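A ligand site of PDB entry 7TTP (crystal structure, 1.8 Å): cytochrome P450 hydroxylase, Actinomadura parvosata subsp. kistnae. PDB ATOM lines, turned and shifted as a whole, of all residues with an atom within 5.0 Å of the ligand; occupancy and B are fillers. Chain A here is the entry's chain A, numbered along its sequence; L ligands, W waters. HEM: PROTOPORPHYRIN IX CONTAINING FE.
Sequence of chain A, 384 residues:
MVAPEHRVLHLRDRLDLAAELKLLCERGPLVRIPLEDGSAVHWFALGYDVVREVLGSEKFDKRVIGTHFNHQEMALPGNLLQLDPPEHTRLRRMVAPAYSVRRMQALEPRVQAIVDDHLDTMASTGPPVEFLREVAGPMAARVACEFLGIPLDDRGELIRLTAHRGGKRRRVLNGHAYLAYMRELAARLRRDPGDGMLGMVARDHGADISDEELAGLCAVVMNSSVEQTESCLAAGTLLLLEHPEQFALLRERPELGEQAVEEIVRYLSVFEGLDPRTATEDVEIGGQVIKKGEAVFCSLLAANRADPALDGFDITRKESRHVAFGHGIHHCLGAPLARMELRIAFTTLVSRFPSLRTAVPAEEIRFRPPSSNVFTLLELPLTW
Water W2 lies within hydrogen-bond range of O2A of the ligand (2.7 Å) and N of Asp 275 (2.8 Å). Water W1 bridges OG of Ser 225 and OG1 of Thr 229.
An oxygen (O2D) of the ligand is in hydrogen-bond range of a ring nitrogen (ND1) of His 330 (2.6 Å). The backbone NH of Leu 81 is in hydrogen-bond range of an oxygen (O2D) of the ligand, 3.5 Å away. SG of Cys 332 binds FE of the ligand, at 2.3 Å. NH2 of Arg 277 is in salt-bridge range of O1A of the ligand (2.8 Å). A ring nitrogen (NE2) of His 88 lies within hydrogen-bond range of an oxygen (O1D) of the ligand (2.7 Å). NH1 of Arg 92 lies within salt-bridge range of O1D of the ligand, 2.8 Å away.
The side-chain amide nitrogen (NE2) of Gln 228 lies close to a nitrogen (NB) of the ligand, 3.0 Å away. Leu 80 touches the ligand (C to O2D, 3.5 Å). Tyr 99 touches the ligand (OH to CAC, 3.6 Å). Val 221 touches the ligand. Ser 225 touches the ligand. OG1 of Thr 229 touches CMC of the ligand (3.7 Å). SG of Cys 232 touches CBB of the ligand (3.1 Å). CD2 of Phe 271 touches CHB of the ligand (3.5 Å). Leu 274 touches the ligand (CD2 to O2A, 3.6 Å). Leu 300 touches the ligand. O of Ala 324 touches CMA of the ligand (3.5 Å). C of Phe 325 touches CMA of the ligand, 3.5 Å away. Gly 326 touches the ligand (N to CMA, 3.5 Å). Ile 329 touches the ligand. Leu 333 touches the ligand (N to ND, 3.8 Å). CA of Gly 334 touches C3C of the ligand (3.4 Å). Leu 337 touches the ligand (CD2 to CBC, 3.6 Å). CB of Ala 338 touches CAB of the ligand (3.98 Å). Hydrophobic or aromatic side chains that line the ligand: Leu 80, Leu 81, His 88, Tyr 99, Val 221, Phe 271, Leu 274, Leu 300, Phe 325, His 330, Leu 333, Leu 337 and Ala 338. Along chain A the residues within 4 Å of the ligand span positions 80 to 338. The nearest printed residue that does not touch the ligand is Val 270 (4.1 Å).
OG1 of Thr 229 sits at hydrogen-bond distance from O of Ser 225 (2.8 Å). A ring nitrogen (NE2) of His 88 sits close to the backbone carbonyl oxygen (O) of Ile 329 (3.5 Å). OG of Ser 225 sits at hydrogen-bond distance from O of Val 221 (2.6 Å). N of Cys 332 sits at hydrogen-bond distance from O of Phe 325 (2.9 Å). O of Ile 329 sits at hydrogen-bond distance from NH1 of Arg 92 (3.2 Å). SG of Cys 332 sits close to N of Gly 334, 3.2 Å away. The backbone carbonyl oxygen (O) of His 331 sits at hydrogen-bond distance from the guanidinium group (NH1) of Arg 92 (2.7 Å). O of Val 220 lies within hydrogen-bond range of N of Ser 225 (3.1 Å).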
ATOM      1  N   LEU A  55      24.006 -10.483   5.808  1.00  0.00           N
ATOM      2  CA  LEU A  55      24.869 -11.583   5.416  1.00  0.00           C
ATOM      3  C   LEU A  55      26.309 -11.417   5.919  1.00  0.00           C
ATOM      4  O   LEU A  55      27.028 -12.417   6.056  1.00  0.00           O
ATOM      5  CB  LEU A  55      24.887 -11.708   3.895  1.00  0.00           C
ATOM      6  CG  LEU A  55      23.572 -12.188   3.271  1.00  0.00           C
ATOM      7  CD1 LEU A  55      23.625 -12.280   1.767  1.00  0.00           C
ATOM      8  CD2 LEU A  55      23.159 -13.562   3.858  1.00  0.00           C
ATOM      9  N   LYS A  62      22.950 -20.460  10.566  1.00  0.00           N
ATOM     10  CA  LYS A  62      22.049 -21.096   9.610  1.00  0.00           C
ATOM     11  C   LYS A  62      21.336 -22.283  10.243  1.00  0.00           C
ATOM     12  O   LYS A  62      21.199 -23.350   9.637  1.00  0.00           O
ATOM     13  CB  LYS A  62      22.816 -21.502   8.347  1.00  0.00           C
ATOM     14  CG  LYS A  62      23.119 -20.286   7.470  1.00  0.00           C
ATOM     15  CD  LYS A  62      23.715 -20.656   6.131  1.00  0.00           C
ATOM     16  CE  LYS A  62      22.642 -20.956   5.100  1.00  0.00           C
ATOM     17  NZ  LYS A  62      22.008 -22.312   5.324  1.00  0.00           N
ATOM     18  N   LEU A  80      28.728 -26.997   2.449  1.00  0.00           N
ATOM     19  CA  LEU A  80      29.177 -25.791   3.160  1.00  0.00           C
ATOM     20  C   LEU A  80      28.003 -24.937   3.626  1.00  0.00           C
ATOM     21  O   LEU A  80      28.090 -24.286   4.667  1.00  0.00           O
ATOM     22  CB  LEU A  80      30.098 -24.968   2.259  1.00  0.00           C
ATOM     23  CG  LEU A  80      31.538 -25.454   2.138  1.00  0.00           C
ATOM     24  CD1 LEU A  80      32.240 -24.820   0.922  1.00  0.00           C
ATOM     25  CD2 LEU A  80      32.289 -25.113   3.409  1.00  0.00           C
ATOM     26  N   LEU A  81      26.920 -24.907   2.851  1.00  0.00           N
ATOM     27  CA  LEU A  81      25.835 -24.007   3.195  1.00  0.00           C
ATOM     28  C   LEU A  81      25.134 -24.382   4.497  1.00  0.00           C
ATOM     29  O   LEU A  81      24.419 -23.547   5.058  1.00  0.00           O
ATOM     30  CB  LEU A  81      24.803 -23.973   2.083  1.00  0.00           C
ATOM     31  CG  LEU A  81      24.831 -22.757   1.163  1.00  0.00           C
ATOM     32  CD1 LEU A  81      23.736 -22.920   0.095  1.00  0.00           C
ATOM     33  CD2 LEU A  81      24.671 -21.474   1.934  1.00  0.00           C
ATOM     34  N   HIS A  88      32.493 -24.545   9.250  1.00  0.00           N
ATOM     35  CA  HIS A  88      32.404 -23.983   7.899  1.00  0.00           C
ATOM     36  C   HIS A  88      33.764 -23.477   7.434  1.00  0.00           C
ATOM     37  O   HIS A  88      34.199 -23.782   6.313  1.00  0.00           O
ATOM     38  CB  HIS A  88      31.382 -22.854   7.890  1.00  0.00           C
ATOM     39  CG  HIS A  88      31.388 -22.060   6.621  1.00  0.00           C
ATOM     40  ND1 HIS A  88      32.130 -20.916   6.461  1.00  0.00           N
ATOM     41  CD2 HIS A  88      30.772 -22.284   5.438  1.00  0.00           C
ATOM     42  CE1 HIS A  88      31.942 -20.441   5.242  1.00  0.00           C
ATOM     43  NE2 HIS A  88      31.121 -21.248   4.600  1.00  0.00           N
ATOM     44  N   ARG A  92      35.725 -24.829   4.101  1.00  0.00           N
ATOM     45  CA  ARG A  92      35.840 -23.883   3.004  1.00  0.00           C
ATOM     46  C   ARG A  92      37.305 -23.586   2.711  1.00  0.00           C
ATOM     47  O   ARG A  92      37.699 -23.488   1.541  1.00  0.00           O
ATOM     48  CB  ARG A  92      35.092 -22.603   3.318  1.00  0.00           C
ATOM     49  CG  ARG A  92      35.140 -21.617   2.160  1.00  0.00           C
ATOM     50  CD  ARG A  92      33.935 -20.725   2.072  1.00  0.00           C
ATOM     51  NE  ARG A  92      34.139 -19.736   1.019  1.00  0.00           N
ATOM     52  CZ  ARG A  92      33.181 -19.215   0.265  1.00  0.00           C
ATOM     53  NH1 ARG A  92      31.909 -19.567   0.427  1.00  0.00           N
ATOM     54  NH2 ARG A  92      33.509 -18.347  -0.692  1.00  0.00           N
ATOM     55  N   TYR A  99      39.428 -22.475  -6.662  1.00  0.00           N
ATOM     56  CA  TYR A  99      38.792 -21.384  -7.397  1.00  0.00           C
ATOM     57  C   TYR A  99      39.669 -20.147  -7.507  1.00  0.00           C
ATOM     58  O   TYR A  99      39.167 -19.065  -7.860  1.00  0.00           O
ATOM     59  CB  TYR A  99      37.448 -20.993  -6.771  1.00  0.00           C
ATOM     60  CG  TYR A  99      36.463 -22.129  -6.640  1.00  0.00           C
ATOM     61  CD1 TYR A  99      36.537 -23.013  -5.571  1.00  0.00           C
ATOM     62  CD2 TYR A  99      35.459 -22.314  -7.582  1.00  0.00           C
ATOM     63  CE1 TYR A  99      35.640 -24.051  -5.449  1.00  0.00           C
ATOM     64  CE2 TYR A  99      34.550 -23.348  -7.456  1.00  0.00           C
ATOM     65  CZ  TYR A  99      34.638 -24.201  -6.382  1.00  0.00           C
ATOM     66  OH  TYR A  99      33.739 -25.229  -6.274  1.00  0.00           O
ATOM     67  N   PHE A 147      35.981 -29.055 -14.368  1.00  0.00           N
ATOM     68  CA  PHE A 147      36.435 -28.368 -13.167  1.00  0.00           C
ATOM     69  C   PHE A 147      36.698 -29.335 -12.015  1.00  0.00           C
ATOM     70  O   PHE A 147      37.691 -29.211 -11.283  1.00  0.00           O
ATOM     71  CB  PHE A 147      35.417 -27.333 -12.741  1.00  0.00           C
ATOM     72  CG  PHE A 147      35.653 -26.812 -11.353  1.00  0.00           C
ATOM     73  CD1 PHE A 147      36.699 -25.936 -11.094  1.00  0.00           C
ATOM     74  CD2 PHE A 147      34.870 -27.223 -10.304  1.00  0.00           C
ATOM     75  CE1 PHE A 147      36.943 -25.461  -9.824  1.00  0.00           C
ATOM     76  CE2 PHE A 147      35.090 -26.737  -9.002  1.00  0.00           C
ATOM     77  CZ  PHE A 147      36.135 -25.863  -8.764  1.00  0.00           C
ATOM     78  N   VAL A 220      27.126 -31.031  -4.720  1.00  0.00           N
ATOM     79  CA  VAL A 220      26.674 -29.639  -4.734  1.00  0.00           C
ATOM     80  C   VAL A 220      27.043 -28.983  -6.054  1.00  0.00           C
ATOM     81  O   VAL A 220      26.270 -28.171  -6.593  1.00  0.00           O
ATOM     82  CB  VAL A 220      27.262 -28.885  -3.522  1.00  0.00           C
ATOM     83  CG1 VAL A 220      27.083 -27.387  -3.695  1.00  0.00           C
ATOM     84  CG2 VAL A 220      26.573 -29.382  -2.242  1.00  0.00           C
ATOM     85  N   VAL A 221      28.220 -29.304  -6.579  1.00  0.00           N
ATOM     86  CA  VAL A 221      28.656 -28.747  -7.864  1.00  0.00           C
ATOM     87  C   VAL A 221      27.803 -29.304  -8.992  1.00  0.00           C
ATOM     88  O   VAL A 221      27.284 -28.553  -9.824  1.00  0.00           O
ATOM     89  CB  VAL A 221      30.158 -29.027  -8.078  1.00  0.00           C
ATOM     90  CG1 VAL A 221      30.596 -28.623  -9.476  1.00  0.00           C
ATOM     91  CG2 VAL A 221      30.970 -28.279  -7.067  1.00  0.00           C
ATOM     92  N   SER A 225      24.555 -26.377  -8.427  1.00  0.00           N
ATOM     93  CA  SER A 225      25.330 -25.377  -9.135  1.00  0.00           C
ATOM     94  C   SER A 225      25.072 -25.442 -10.636  1.00  0.00           C
ATOM     95  O   SER A 225      24.950 -24.394 -11.274  1.00  0.00           O
ATOM     96  CB  SER A 225      26.825 -25.534  -8.820  1.00  0.00           C
ATOM     97  OG  SER A 225      27.575 -25.945  -9.941  1.00  0.00           O
ATOM     98  N   GLN A 228      21.663 -23.831 -11.288  1.00  0.00           N
ATOM     99  CA  GLN A 228      21.794 -22.379 -11.349  1.00  0.00           C
ATOM    100  C   GLN A 228      22.516 -21.943 -12.613  1.00  0.00           C
ATOM    101  O   GLN A 228      22.105 -20.971 -13.260  1.00  0.00           O
ATOM    102  CB  GLN A 228      22.528 -21.898 -10.106  1.00  0.00           C
ATOM    103  CG  GLN A 228      21.715 -22.189  -8.822  1.00  0.00           C
ATOM    104  CD  GLN A 228      22.547 -22.451  -7.617  1.00  0.00           C
ATOM    105  OE1 GLN A 228      22.052 -22.986  -6.618  1.00  0.00           O
ATOM    106  NE2 GLN A 228      23.807 -22.055  -7.670  1.00  0.00           N
ATOM    107  N   THR A 229      23.600 -22.636 -12.969  1.00  0.00           N
ATOM    108  CA  THR A 229      24.381 -22.219 -14.127  1.00  0.00           C
ATOM    109  C   THR A 229      23.592 -22.433 -15.411  1.00  0.00           C
ATOM    110  O   THR A 229      23.559 -21.551 -16.276  1.00  0.00           O
ATOM    111  CB  THR A 229      25.720 -22.969 -14.160  1.00  0.00           C
ATOM    112  OG1 THR A 229      26.411 -22.722 -12.930  1.00  0.00           O
ATOM    113  CG2 THR A 229      26.556 -22.485 -15.323  1.00  0.00           C
ATOM    114  N   CYS A 232      21.022 -19.729 -15.758  1.00  0.00           N
ATOM    115  CA  CYS A 232      21.606 -18.471 -16.217  1.00  0.00           C
ATOM    116  C   CYS A 232      21.886 -18.523 -17.713  1.00  0.00           C
ATOM    117  O   CYS A 232      21.589 -17.569 -18.439  1.00  0.00           O
ATOM    118  CB  CYS A 232      22.902 -18.158 -15.464  1.00  0.00           C
ATOM    119  SG  CYS A 232      22.733 -17.547 -13.785  1.00  0.00           S
ATOM    120  N   VAL A 265      23.420 -11.797 -14.346  1.00  0.00           N
ATOM    121  CA  VAL A 265      23.107 -12.493 -13.090  1.00  0.00           C
ATOM    122  C   VAL A 265      22.282 -11.590 -12.162  1.00  0.00           C
ATOM    123  O   VAL A 265      21.389 -12.080 -11.453  1.00  0.00           O
ATOM    124  CB  VAL A 265      24.372 -13.033 -12.375  1.00  0.00           C
ATOM    125  CG1 VAL A 265      25.085 -14.011 -13.252  1.00  0.00           C
ATOM    126  CG2 VAL A 265      25.308 -11.902 -11.944  1.00  0.00           C
ATOM    127  N   VAL A 270      18.614 -15.866 -10.450  1.00  0.00           N
ATOM    128  CA  VAL A 270      18.057 -17.223 -10.493  1.00  0.00           C
ATOM    129  C   VAL A 270      18.056 -17.836  -9.100  1.00  0.00           C
ATOM    130  O   VAL A 270      17.181 -18.656  -8.782  1.00  0.00           O
ATOM    131  CB  VAL A 270      18.819 -18.119 -11.484  1.00  0.00           C
ATOM    132  CG1 VAL A 270      18.825 -17.503 -12.868  1.00  0.00           C
ATOM    133  CG2 VAL A 270      20.235 -18.385 -11.005  1.00  0.00           C
ATOM    134  N   PHE A 271      19.002 -17.444  -8.247  1.00  0.00           N
ATOM    135  CA  PHE A 271      18.992 -17.795  -6.835  1.00  0.00           C
ATOM    136  C   PHE A 271      18.252 -16.646  -6.182  1.00  0.00           C
ATOM    137  O   PHE A 271      18.822 -15.574  -5.963  1.00  0.00           O
ATOM    138  CB  PHE A 271      20.412 -17.953  -6.325  1.00  0.00           C
ATOM    139  CG  PHE A 271      20.563 -18.798  -5.121  1.00  0.00           C
ATOM    140  CD1 PHE A 271      19.647 -18.718  -4.068  1.00  0.00           C
ATOM    141  CD2 PHE A 271      21.665 -19.608  -4.983  1.00  0.00           C
ATOM    142  CE1 PHE A 271      19.829 -19.454  -2.907  1.00  0.00           C
ATOM    143  CE2 PHE A 271      21.856 -20.372  -3.794  1.00  0.00           C
ATOM    144  CZ  PHE A 271      20.921 -20.295  -2.788  1.00  0.00           C
ATOM    145  N   LEU A 274      17.435 -16.612   0.012  1.00  0.00           N
ATOM    146  CA  LEU A 274      18.391 -17.400   0.766  1.00  0.00           C
ATOM    147  C   LEU A 274      17.748 -18.106   1.952  1.00  0.00           C
ATOM    148  O   LEU A 274      16.703 -17.696   2.483  1.00  0.00           O
ATOM    149  CB  LEU A 274      19.549 -16.530   1.266  1.00  0.00           C
ATOM    150  CG  LEU A 274      20.341 -15.766   0.217  1.00  0.00           C
ATOM    151  CD1 LEU A 274      21.534 -15.075   0.927  1.00  0.00           C
ATOM    152  CD2 LEU A 274      20.818 -16.694  -0.873  1.00  0.00           C
ATOM    153  N   ASP A 275      18.411 -19.219   2.373  1.00  0.00           N
ATOM    154  CA  ASP A 275      18.125 -19.923   3.605  1.00  0.00           C
ATOM    155  C   ASP A 275      18.095 -18.874   4.710  1.00  0.00           C
ATOM    156  O   ASP A 275      18.923 -17.941   4.675  1.00  0.00           O
ATOM    157  CB  ASP A 275      19.187 -20.957   3.963  1.00  0.00           C
ATOM    158  CG  ASP A 275      19.263 -22.078   2.977  1.00  0.00           C
ATOM    159  OD1 ASP A 275      18.242 -22.355   2.314  1.00  0.00           O
ATOM    160  OD2 ASP A 275      20.360 -22.694   2.883  1.00  0.00           O
ATOM    161  N   ARG A 277      18.652 -16.713   8.077  1.00  0.00           N
ATOM    162  CA  ARG A 277      19.706 -16.405   9.033  1.00  0.00           C
ATOM    163  C   ARG A 277      19.035 -16.090  10.359  1.00  0.00           C
ATOM    164  O   ARG A 277      18.226 -15.169  10.429  1.00  0.00           O
ATOM    165  CB  ARG A 277      20.543 -15.219   8.570  1.00  0.00           C
ATOM    166  CG  ARG A 277      21.839 -15.606   7.862  1.00  0.00           C
ATOM    167  CD  ARG A 277      21.624 -16.366   6.583  1.00  0.00           C
ATOM    168  NE  ARG A 277      22.886 -16.563   5.897  1.00  0.00           N
ATOM    169  CZ  ARG A 277      23.011 -17.087   4.686  1.00  0.00           C
ATOM    170  NH1 ARG A 277      21.967 -17.551   4.018  1.00  0.00           N
ATOM    171  NH2 ARG A 277      24.219 -17.171   4.143  1.00  0.00           N
ATOM    172  N   LEU A 300      17.439 -11.939  -2.618  1.00  0.00           N
ATOM    173  CA  LEU A 300      18.362 -11.444  -3.617  1.00  0.00           C
ATOM    174  C   LEU A 300      17.599 -10.850  -4.774  1.00  0.00           C
ATOM    175  O   LEU A 300      18.017  -9.844  -5.353  1.00  0.00           O
ATOM    176  CB  LEU A 300      19.281 -12.564  -4.115  1.00  0.00           C
ATOM    177  CG  LEU A 300      19.962 -13.346  -2.990  1.00  0.00           C
ATOM    178  CD1 LEU A 300      20.966 -14.327  -3.582  1.00  0.00           C
ATOM    179  CD2 LEU A 300      20.695 -12.401  -1.994  1.00  0.00           C
ATOM    180  N   VAL A 323      23.654  -8.613  -5.459  1.00  0.00           N
ATOM    181  CA  VAL A 323      24.040  -9.657  -4.511  1.00  0.00           C
ATOM    182  C   VAL A 323      23.674 -11.029  -5.066  1.00  0.00           C
ATOM    183  O   VAL A 323      23.327 -11.939  -4.297  1.00  0.00           O
ATOM    184  CB  VAL A 323      23.365  -9.435  -3.149  1.00  0.00           C
ATOM    185  CG1 VAL A 323      23.962  -8.246  -2.452  1.00  0.00           C
ATOM    186  CG2 VAL A 323      21.858  -9.231  -3.297  1.00  0.00           C
ATOM    187  N   ALA A 324      23.800 -11.197  -6.379  1.00  0.00           N
ATOM    188  CA  ALA A 324      23.332 -12.435  -7.009  1.00  0.00           C
ATOM    189  C   ALA A 324      24.109 -13.653  -6.530  1.00  0.00           C
ATOM    190  O   ALA A 324      23.597 -14.776  -6.595  1.00  0.00           O
ATOM    191  CB  ALA A 324      23.411 -12.351  -8.530  1.00  0.00           C
ATOM    192  N   PHE A 325      25.369 -13.467  -6.092  1.00  0.00           N
ATOM    193  CA  PHE A 325      26.198 -14.536  -5.539  1.00  0.00           C
ATOM    194  C   PHE A 325      26.300 -14.457  -4.018  1.00  0.00           C
ATOM    195  O   PHE A 325      27.179 -15.100  -3.428  1.00  0.00           O
ATOM    196  CB  PHE A 325      27.611 -14.479  -6.122  1.00  0.00           C
ATOM    197  CG  PHE A 325      27.684 -14.823  -7.583  1.00  0.00           C
ATOM    198  CD1 PHE A 325      27.436 -16.109  -8.005  1.00  0.00           C
ATOM    199  CD2 PHE A 325      28.037 -13.859  -8.527  1.00  0.00           C
ATOM    200  CE1 PHE A 325      27.536 -16.457  -9.359  1.00  0.00           C
ATOM    201  CE2 PHE A 325      28.110 -14.186  -9.864  1.00  0.00           C
ATOM    202  CZ  PHE A 325      27.863 -15.484 -10.293  1.00  0.00           C
ATOM    203  N   GLY A 326      25.428 -13.709  -3.366  1.00  0.00           N
ATOM    204  CA  GLY A 326      25.462 -13.593  -1.930  1.00  0.00           C
ATOM    205  C   GLY A 326      26.565 -12.651  -1.450  1.00  0.00           C
ATOM    206  O   GLY A 326      27.068 -11.788  -2.190  1.00  0.00           O
ATOM    207  N   ILE A 329      30.593 -14.862   4.581  1.00  0.00           N
ATOM    208  CA  ILE A 329      31.391 -16.087   4.601  1.00  0.00           C
ATOM    209  C   ILE A 329      30.830 -17.160   3.688  1.00  0.00           C
ATOM    210  O   ILE A 329      31.564 -18.059   3.271  1.00  0.00           O
ATOM    211  CB  ILE A 329      31.537 -16.636   6.023  1.00  0.00           C
ATOM    212  CG1 ILE A 329      30.177 -16.964   6.603  1.00  0.00           C
ATOM    213  CG2 ILE A 329      32.263 -15.630   6.906  1.00  0.00           C
ATOM    214  CD1 ILE A 329      30.234 -17.787   7.956  1.00  0.00           C
ATOM    215  N   HIS A 330      29.529 -17.109   3.391  1.00  0.00           N
ATOM    216  CA  HIS A 330      28.879 -18.081   2.526  1.00  0.00           C
ATOM    217  C   HIS A 330      28.796 -17.612   1.074  1.00  0.00           C
ATOM    218  O   HIS A 330      28.161 -18.285   0.250  1.00  0.00           O
ATOM    219  CB  HIS A 330      27.468 -18.406   3.037  1.00  0.00           C
ATOM    220  CG  HIS A 330      27.439 -19.238   4.285  1.00  0.00           C
ATOM    221  ND1 HIS A 330      27.670 -20.597   4.298  1.00  0.00           N
ATOM    222  CD2 HIS A 330      27.194 -18.885   5.573  1.00  0.00           C
ATOM    223  CE1 HIS A 330      27.566 -21.044   5.545  1.00  0.00           C
ATOM    224  NE2 HIS A 330      27.318 -20.019   6.335  1.00  0.00           N
ATOM    225  N   HIS A 331      29.394 -16.467   0.754  1.00  0.00           N
ATOM    226  CA  HIS A 331      29.452 -15.983  -0.623  1.00  0.00           C
ATOM    227  C   HIS A 331      29.790 -17.113  -1.591  1.00  0.00           C
ATOM    228  O   HIS A 331      30.748 -17.866  -1.385  1.00  0.00           O
ATOM    229  CB  HIS A 331      30.502 -14.878  -0.743  1.00  0.00           C
ATOM    230  CG  HIS A 331      30.633 -14.305  -2.120  1.00  0.00           C
ATOM    231  ND1 HIS A 331      31.489 -14.843  -3.063  1.00  0.00           N
ATOM    232  CD2 HIS A 331      30.013 -13.268  -2.726  1.00  0.00           C
ATOM    233  CE1 HIS A 331      31.390 -14.150  -4.181  1.00  0.00           C
ATOM    234  NE2 HIS A 331      30.510 -13.184  -4.006  1.00  0.00           N
ATOM    235  N   CYS A 332      29.085 -17.144  -2.712  1.00  0.00           N
ATOM    236  CA  CYS A 332      29.208 -18.270  -3.638  1.00  0.00           C
ATOM    237  C   CYS A 332      30.651 -18.657  -3.902  1.00  0.00           C
ATOM    238  O   CYS A 332      31.451 -17.878  -4.427  1.00  0.00           O
ATOM    239  CB  CYS A 332      28.541 -17.940  -4.954  1.00  0.00           C
ATOM    240  SG  CYS A 332      28.742 -19.344  -6.132  1.00  0.00           S
ATOM    241  N   LEU A 333      31.003 -19.882  -3.490  1.00  0.00           N
ATOM    242  CA  LEU A 333      32.366 -20.359  -3.692  1.00  0.00           C
ATOM    243  C   LEU A 333      32.667 -20.537  -5.179  1.00  0.00           C
ATOM    244  O   LEU A 333      33.821 -20.405  -5.615  1.00  0.00           O
ATOM    245  CB  LEU A 333      32.557 -21.663  -2.929  1.00  0.00           C
ATOM    246  CG  LEU A 333      33.922 -22.299  -2.838  1.00  0.00           C
ATOM    247  CD1 LEU A 333      34.892 -21.380  -2.149  1.00  0.00           C
ATOM    248  CD2 LEU A 333      33.826 -23.644  -2.109  1.00  0.00           C
ATOM    249  N   GLY A 334      31.636 -20.813  -5.968  1.00  0.00           N
ATOM    250  CA  GLY A 334      31.805 -21.053  -7.386  1.00  0.00           C
ATOM    251  C   GLY A 334      31.778 -19.833  -8.266  1.00  0.00           C
ATOM    252  O   GLY A 334      31.882 -19.930  -9.498  1.00  0.00           O
ATOM    253  N   LEU A 337      34.169 -19.494 -11.216  1.00  0.00           N
ATOM    254  CA  LEU A 337      33.895 -20.418 -12.311  1.00  0.00           C
ATOM    255  C   LEU A 337      32.645 -19.986 -13.067  1.00  0.00           C
ATOM    256  O   LEU A 337      32.636 -19.987 -14.308  1.00  0.00           O
ATOM    257  CB  LEU A 337      33.734 -21.832 -11.760  1.00  0.00           C
ATOM    258  CG  LEU A 337      33.386 -22.889 -12.779  1.00  0.00           C
ATOM    259  CD1 LEU A 337      34.468 -23.012 -13.859  1.00  0.00           C
ATOM    260  CD2 LEU A 337      33.162 -24.217 -12.083  1.00  0.00           C
ATOM    261  N   ALA A 338      31.567 -19.703 -12.343  1.00  0.00           N
ATOM    262  CA  ALA A 338      30.330 -19.259 -12.980  1.00  0.00           C
ATOM    263  C   ALA A 338      30.558 -18.015 -13.827  1.00  0.00           C
ATOM    264  O   ALA A 338      30.095 -17.930 -14.975  1.00  0.00           O
ATOM    265  CB  ALA A 338      29.274 -19.016 -11.886  1.00  0.00           C
ATOM    266  N   LEU A 342      30.033 -18.322 -17.867  1.00  0.00           N
ATOM    267  CA  LEU A 342      28.983 -17.537 -18.511  1.00  0.00           C
ATOM    268  C   LEU A 342      29.578 -16.538 -19.503  1.00  0.00           C
ATOM    269  O   LEU A 342      29.030 -16.337 -20.587  1.00  0.00           O
ATOM    270  CB  LEU A 342      28.143 -16.822 -17.449  1.00  0.00           C
ATOM    271  CG  LEU A 342      27.367 -17.731 -16.488  1.00  0.00           C
ATOM    272  CD1 LEU A 342      26.657 -16.905 -15.405  1.00  0.00           C
ATOM    273  CD2 LEU A 342      26.338 -18.574 -17.292  1.00  0.00           C
HETATM  274  CHA HEM L   1      26.763 -20.467  -2.447  1.00  0.00           C
HETATM  275  CHB HEM L   1      24.614 -18.290  -6.203  1.00  0.00           C
HETATM  276  CHC HEM L   1      27.049 -21.162  -9.275  1.00  0.00           C
HETATM  277  CHD HEM L   1      29.130 -23.412  -5.517  1.00  0.00           C
HETATM  278  C1A HEM L   1      25.995 -19.591  -3.191  1.00  0.00           C
HETATM  279  C2A HEM L   1      25.172 -18.508  -2.683  1.00  0.00           C
HETATM  280  C3A HEM L   1      24.574 -17.905  -3.718  1.00  0.00           C
HETATM  281  C4A HEM L   1      25.013 -18.593  -4.919  1.00  0.00           C
HETATM  282  CMA HEM L   1      23.590 -16.717  -3.685  1.00  0.00           C
HETATM  283  CAA HEM L   1      25.016 -18.107  -1.199  1.00  0.00           C
HETATM  284  CBA HEM L   1      23.821 -18.798  -0.555  1.00  0.00           C
HETATM  285  CGA HEM L   1      23.632 -18.326   0.863  1.00  0.00           C
HETATM  286  O1A HEM L   1      24.463 -17.541   1.389  1.00  0.00           O
HETATM  287  O2A HEM L   1      22.619 -18.750   1.494  1.00  0.00           O
HETATM  288  C1B HEM L   1      25.083 -18.877  -7.361  1.00  0.00           C
HETATM  289  C2B HEM L   1      24.689 -18.517  -8.727  1.00  0.00           C
HETATM  290  C3B HEM L   1      25.348 -19.339  -9.560  1.00  0.00           C
HETATM  291  C4B HEM L   1      26.182 -20.208  -8.758  1.00  0.00           C
HETATM  292  CMB HEM L   1      23.712 -17.352  -9.057  1.00  0.00           C
HETATM  293  CAB HEM L   1      25.385 -19.384 -11.106  1.00  0.00           C
HETATM  294  CBB HEM L   1      25.084 -18.306 -11.838  1.00  0.00           C
HETATM  295  C1C HEM L   1      27.874 -21.957  -8.520  1.00  0.00           C
HETATM  296  C2C HEM L   1      28.917 -22.820  -9.044  1.00  0.00           C
HETATM  297  C3C HEM L   1      29.481 -23.453  -8.004  1.00  0.00           C
HETATM  298  C4C HEM L   1      28.824 -22.997  -6.794  1.00  0.00           C
HETATM  299  CMC HEM L   1      29.274 -22.954 -10.552  1.00  0.00           C
HETATM  300  CAC HEM L   1      30.648 -24.474  -7.957  1.00  0.00           C
HETATM  301  CBC HEM L   1      31.298 -24.884  -9.048  1.00  0.00           C
HETATM  302  C1D HEM L   1      28.630 -22.843  -4.359  1.00  0.00           C
HETATM  303  C2D HEM L   1      28.946 -23.261  -3.014  1.00  0.00           C
HETATM  304  C3D HEM L   1      28.279 -22.466  -2.157  1.00  0.00           C
HETATM  305  C4D HEM L   1      27.536 -21.497  -2.946  1.00  0.00           C
HETATM  306  CMD HEM L   1      29.846 -24.458  -2.667  1.00  0.00           C
HETATM  307  CAD HEM L   1      28.274 -22.518  -0.604  1.00  0.00           C
HETATM  308  CBD HEM L   1      29.393 -21.633  -0.053  1.00  0.00           C
HETATM  309  CGD HEM L   1      29.356 -21.567   1.451  1.00  0.00           C
HETATM  310  O1D HEM L   1      30.403 -21.278   2.049  1.00  0.00           O
HETATM  311  O2D HEM L   1      28.294 -21.824   2.049  1.00  0.00           O
HETATM  312  NA  HEM L   1      25.874 -19.604  -4.558  1.00  0.00           N
HETATM  313  NB  HEM L   1      25.973 -19.925  -7.417  1.00  0.00           N
HETATM  314  NC  HEM L   1      27.843 -22.089  -7.138  1.00  0.00           N
HETATM  315  ND  HEM L   1      27.774 -21.752  -4.300  1.00  0.00           N
HETATM  316 FE   HEM L   1      26.965 -20.762  -5.870  1.00  0.00          FE
HETATM  317  O   HOH W   1      27.803 -25.244 -12.613  1.00  0.00           O
HETATM  318  O   HOH W   2      20.488 -20.297   0.875  1.00  0.00           O
HETATM  319  O   HOH W   3      26.042 -15.422   0.996  1.00  0.00           O
